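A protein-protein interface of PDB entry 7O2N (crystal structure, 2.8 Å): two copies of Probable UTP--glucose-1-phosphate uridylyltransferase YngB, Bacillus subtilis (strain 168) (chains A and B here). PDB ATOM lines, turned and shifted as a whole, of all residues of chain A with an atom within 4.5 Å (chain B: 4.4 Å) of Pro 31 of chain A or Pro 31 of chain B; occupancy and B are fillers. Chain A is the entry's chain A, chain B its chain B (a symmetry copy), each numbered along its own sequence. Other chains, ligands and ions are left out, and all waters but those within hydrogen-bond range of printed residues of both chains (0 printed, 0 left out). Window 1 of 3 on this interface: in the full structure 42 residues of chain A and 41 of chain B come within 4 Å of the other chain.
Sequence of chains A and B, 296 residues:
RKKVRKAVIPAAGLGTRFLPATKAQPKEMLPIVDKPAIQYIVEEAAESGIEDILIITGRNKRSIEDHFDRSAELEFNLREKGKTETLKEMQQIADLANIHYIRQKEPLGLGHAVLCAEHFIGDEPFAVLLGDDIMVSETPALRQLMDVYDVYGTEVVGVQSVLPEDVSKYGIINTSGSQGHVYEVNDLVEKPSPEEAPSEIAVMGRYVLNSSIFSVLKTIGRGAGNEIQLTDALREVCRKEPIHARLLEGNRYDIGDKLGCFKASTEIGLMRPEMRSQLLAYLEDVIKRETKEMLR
Printed residues of chain B within 4 Å of Ala 21 of chain A: Pro 31 (3.9 Å). Of the printed residues of chain B, Leu 30 of chain A touches Pro 31. Pro 31 of chain A touches just one residue of chain B: Pro 31 (3.8 Å). Val 33 of chain A touches none of the printed residues of chain B. Of the printed residues of chain A, Pro 31 of chain B touches Ala 21 (3.9 Å), Leu 30 (3.8 Å) and Pro 31 (3.8 Å). The nearest residue of chain B that does not touch Pro 31 of chain A is Ala 21 of chain B (4.1 Å). The nearest printed residue of chain A that does not touch Pro 31 of chain B is Met 29 of chain A (6.6 Å). The nearest printed residue of chain B that does not touch Leu 30 of chain A is Met 29 of chain B (6.2 Å).
CB of Pro 31 of chain B touches CB of Ala 21 of chain A (3.9 Å). Leu 30 of chain A touches Pro 31 of chain B (CD2 to CG, 3.8 Å). Pro 31 of chain B touches Pro 31 of chain A.
Printed residues of chain B that touch a printed residue of chain A: Pro 31. Hydrophobic or aromatic side chains of chain B that line the printed part of chain A: Pro 31. Among the printed residues, 3 pairs touch across the chains. Among the printed residues, no Asp or Glu carboxylate lies within 4 Å of a Lys or Arg side-chain nitrogen of the other chain.
Ala 21 of chain A touches Pro 31 of chain B, but with the chains exchanged Pro 31 of chain A does not touch Ala 21 of chain B (4.1 Å). Leu 30 of chain A touches Pro 31 of chain B, but with the chains exchanged Pro 31 of chain A does not touch Leu 30 of chain B (4.2 Å). Pro 31 of chain B touches its own counterpart, Pro 31 of chain A. Positions printed for both chains: 21, 29, 30, 31, 32, 33, 35 and 36. Of the 3 pairs that touch across the chains among the printed residues, 1 has its exchanged pair printed and touching as well.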
ATOM      1  N   ALA A  21      10.108 -36.560 -13.166  1.00  0.00           N
ATOM      2  CA  ALA A  21       9.800 -35.145 -12.960  1.00  0.00           C
ATOM      3  C   ALA A  21       9.634 -34.456 -14.305  1.00  0.00           C
ATOM      4  O   ALA A  21       8.659 -33.721 -14.484  1.00  0.00           O
ATOM      5  CB  ALA A  21      10.882 -34.457 -12.168  1.00  0.00           C
ATOM      6  N   MET A  29      13.480 -25.954 -15.909  1.00  0.00           N
ATOM      7  CA  MET A  29      12.510 -25.302 -15.039  1.00  0.00           C
ATOM      8  C   MET A  29      12.485 -25.965 -13.670  1.00  0.00           C
ATOM      9  O   MET A  29      11.808 -25.491 -12.783  1.00  0.00           O
ATOM     10  CB  MET A  29      11.094 -25.339 -15.624  1.00  0.00           C
ATOM     11  CG  MET A  29      10.871 -24.424 -16.805  1.00  0.00           C
ATOM     12  SD  MET A  29      11.339 -22.704 -16.456  1.00  0.00           S
ATOM     13  CE  MET A  29       9.933 -22.186 -15.482  1.00  0.00           C
ATOM     14  N   LEU A  30      13.200 -27.074 -13.494  1.00  0.00           N
ATOM     15  CA  LEU A  30      13.236 -27.715 -12.188  1.00  0.00           C
ATOM     16  C   LEU A  30      13.762 -26.724 -11.159  1.00  0.00           C
ATOM     17  O   LEU A  30      14.712 -25.959 -11.376  1.00  0.00           O
ATOM     18  CB  LEU A  30      14.081 -28.990 -12.222  1.00  0.00           C
ATOM     19  CG  LEU A  30      13.488 -30.136 -13.042  1.00  0.00           C
ATOM     20  CD1 LEU A  30      14.524 -31.227 -13.249  1.00  0.00           C
ATOM     21  CD2 LEU A  30      12.275 -30.714 -12.332  1.00  0.00           C
ATOM     22  N   PRO A  31      13.091 -26.676 -10.000  1.00  0.00           N
ATOM     23  CA  PRO A  31      13.412 -25.672  -8.996  1.00  0.00           C
ATOM     24  C   PRO A  31      14.749 -26.071  -8.376  1.00  0.00           C
ATOM     25  O   PRO A  31      14.994 -27.252  -8.167  1.00  0.00           O
ATOM     26  CB  PRO A  31      12.218 -25.775  -8.033  1.00  0.00           C
ATOM     27  CG  PRO A  31      11.749 -27.215  -8.160  1.00  0.00           C
ATOM     28  CD  PRO A  31      11.988 -27.565  -9.614  1.00  0.00           C
ATOM     29  N   ILE A  32      15.611 -25.081  -8.117  1.00  0.00           N
ATOM     30  CA  ILE A  32      16.808 -25.379  -7.367  1.00  0.00           C
ATOM     31  C   ILE A  32      16.633 -24.985  -5.914  1.00  0.00           C
ATOM     32  O   ILE A  32      16.670 -25.867  -5.056  1.00  0.00           O
ATOM     33  CB  ILE A  32      18.097 -24.886  -8.022  1.00  0.00           C
ATOM     34  CG1 ILE A  32      18.532 -25.895  -9.090  1.00  0.00           C
ATOM     35  CG2 ILE A  32      19.180 -24.689  -6.969  1.00  0.00           C
ATOM     36  CD1 ILE A  32      18.338 -27.346  -8.693  1.00  0.00           C
ATOM     37  N   VAL A  33      16.429 -23.706  -5.591  1.00  0.00           N
ATOM     38  CA  VAL A  33      15.883 -23.638  -4.242  1.00  0.00           C
ATOM     39  C   VAL A  33      14.364 -23.491  -4.350  1.00  0.00           C
ATOM     40  O   VAL A  33      13.589 -24.326  -3.886  1.00  0.00           O
ATOM     41  CB  VAL A  33      16.580 -22.606  -3.345  1.00  0.00           C
ATOM     42  CG1 VAL A  33      15.776 -22.274  -2.089  1.00  0.00           C
ATOM     43  CG2 VAL A  33      17.966 -23.091  -2.989  1.00  0.00           C
ATOM     44  N   LYS A  35      13.824 -21.354  -7.247  1.00  0.00           N
ATOM     45  CA  LYS A  35      14.071 -20.758  -8.542  1.00  0.00           C
ATOM     46  C   LYS A  35      14.320 -21.864  -9.560  1.00  0.00           C
ATOM     47  O   LYS A  35      15.053 -22.831  -9.308  1.00  0.00           O
ATOM     48  CB  LYS A  35      15.347 -19.928  -8.484  1.00  0.00           C
ATOM     49  CG  LYS A  35      15.359 -18.976  -7.314  1.00  0.00           C
ATOM     50  CD  LYS A  35      15.874 -17.637  -7.694  1.00  0.00           C
ATOM     51  CE  LYS A  35      17.350 -17.645  -7.990  1.00  0.00           C
ATOM     52  NZ  LYS A  35      17.830 -16.251  -7.927  1.00  0.00           N
ATOM     53  N   PRO A  36      13.721 -21.735 -10.763  1.00  0.00           N
ATOM     54  CA  PRO A  36      14.037 -22.627 -11.874  1.00  0.00           C
ATOM     55  C   PRO A  36      15.517 -22.482 -12.213  1.00  0.00           C
ATOM     56  O   PRO A  36      16.072 -21.388 -12.179  1.00  0.00           O
ATOM     57  CB  PRO A  36      13.149 -22.080 -12.996  1.00  0.00           C
ATOM     58  CG  PRO A  36      11.998 -21.466 -12.243  1.00  0.00           C
ATOM     59  CD  PRO A  36      12.682 -20.757 -11.100  1.00  0.00           C
ATOM     60  N   ALA B  21       9.208 -20.573  -8.249  1.00  0.00           N
ATOM     61  CA  ALA B  21       9.155 -21.860  -8.942  1.00  0.00           C
ATOM     62  C   ALA B  21       7.868 -21.958  -9.753  1.00  0.00           C
ATOM     63  O   ALA B  21       7.896 -22.393 -10.912  1.00  0.00           O
ATOM     64  CB  ALA B  21       9.243 -23.011  -7.980  1.00  0.00           C
ATOM     65  N   MET B  29       2.958 -29.977  -9.973  1.00  0.00           N
ATOM     66  CA  MET B  29       3.973 -30.623 -10.794  1.00  0.00           C
ATOM     67  C   MET B  29       5.352 -30.506 -10.149  1.00  0.00           C
ATOM     68  O   MET B  29       6.312 -31.076 -10.659  1.00  0.00           O
ATOM     69  CB  MET B  29       4.045 -30.021 -12.199  1.00  0.00           C
ATOM     70  CG  MET B  29       2.904 -30.396 -13.110  1.00  0.00           C
ATOM     71  SD  MET B  29       2.621 -32.174 -13.182  1.00  0.00           S
ATOM     72  CE  MET B  29       3.919 -32.637 -14.319  1.00  0.00           C
ATOM     73  N   LEU B  30       5.474 -29.750  -9.055  1.00  0.00           N
ATOM     74  CA  LEU B  30       6.767 -29.609  -8.398  1.00  0.00           C
ATOM     75  C   LEU B  30       7.269 -30.992  -7.997  1.00  0.00           C
ATOM     76  O   LEU B  30       6.530 -31.848  -7.493  1.00  0.00           O
ATOM     77  CB  LEU B  30       6.684 -28.667  -7.194  1.00  0.00           C
ATOM     78  CG  LEU B  30       6.404 -27.200  -7.514  1.00  0.00           C
ATOM     79  CD1 LEU B  30       6.065 -26.426  -6.248  1.00  0.00           C
ATOM     80  CD2 LEU B  30       7.587 -26.545  -8.203  1.00  0.00           C
ATOM     81  N   PRO B  31       8.552 -31.276  -8.280  1.00  0.00           N
ATOM     82  CA  PRO B  31       9.082 -32.621  -8.080  1.00  0.00           C
ATOM     83  C   PRO B  31       9.228 -32.852  -6.584  1.00  0.00           C
ATOM     84  O   PRO B  31       9.636 -31.935  -5.877  1.00  0.00           O
ATOM     85  CB  PRO B  31      10.415 -32.560  -8.828  1.00  0.00           C
ATOM     86  CG  PRO B  31      10.816 -31.111  -8.806  1.00  0.00           C
ATOM     87  CD  PRO B  31       9.528 -30.320  -8.822  1.00  0.00           C
ATOM     88  N   ILE B  32       8.861 -34.048  -6.109  1.00  0.00           N
ATOM     89  CA  ILE B  32       9.067 -34.329  -4.700  1.00  0.00           C
ATOM     90  C   ILE B  32      10.333 -35.136  -4.466  1.00  0.00           C
ATOM     91  O   ILE B  32      11.256 -34.650  -3.819  1.00  0.00           O
ATOM     92  CB  ILE B  32       7.830 -34.841  -3.956  1.00  0.00           C
ATOM     93  CG1 ILE B  32       6.957 -33.642  -3.577  1.00  0.00           C
ATOM     94  CG2 ILE B  32       8.225 -35.644  -2.726  1.00  0.00           C
ATOM     95  CD1 ILE B  32       7.729 -32.433  -3.074  1.00  0.00           C
ATOM     96  N   VAL B  33      10.454 -36.328  -5.018  1.00  0.00           N
ATOM     97  CA  VAL B  33      11.867 -36.691  -5.096  1.00  0.00           C
ATOM     98  C   VAL B  33      12.342 -36.369  -6.512  1.00  0.00           C
ATOM     99  O   VAL B  33      13.232 -35.568  -6.733  1.00  0.00           O
ATOM    100  CB  VAL B  33      12.142 -38.127  -4.616  1.00  0.00           C
ATOM    101  CG1 VAL B  33      13.488 -38.646  -5.063  1.00  0.00           C
ATOM    102  CG2 VAL B  33      12.019 -38.210  -3.106  1.00  0.00           C
ATOM    103  N   LYS B  35       9.524 -37.157  -8.674  1.00  0.00           N
ATOM    104  CA  LYS B  35       8.131 -37.334  -9.040  1.00  0.00           C
ATOM    105  C   LYS B  35       7.348 -36.052  -8.767  1.00  0.00           C
ATOM    106  O   LYS B  35       7.477 -35.451  -7.700  1.00  0.00           O
ATOM    107  CB  LYS B  35       7.506 -38.379  -8.127  1.00  0.00           C
ATOM    108  CG  LYS B  35       7.578 -39.793  -8.628  1.00  0.00           C
ATOM    109  CD  LYS B  35       6.367 -40.532  -8.167  1.00  0.00           C
ATOM    110  CE  LYS B  35       6.649 -41.409  -6.969  1.00  0.00           C
ATOM    111  NZ  LYS B  35       6.150 -42.800  -7.157  1.00  0.00           N
ATOM    112  N   PRO B  36       6.495 -35.606  -9.706  1.00  0.00           N
ATOM    113  CA  PRO B  36       5.577 -34.500  -9.455  1.00  0.00           C
ATOM    114  C   PRO B  36       4.629 -34.863  -8.320  1.00  0.00           C
ATOM    115  O   PRO B  36       4.202 -36.018  -8.189  1.00  0.00           O
ATOM    116  CB  PRO B  36       4.781 -34.401 -10.748  1.00  0.00           C
ATOM    117  CG  PRO B  36       5.735 -34.964 -11.764  1.00  0.00           C
ATOM    118  CD  PRO B  36       6.382 -36.144 -11.065  1.00  0.00           C
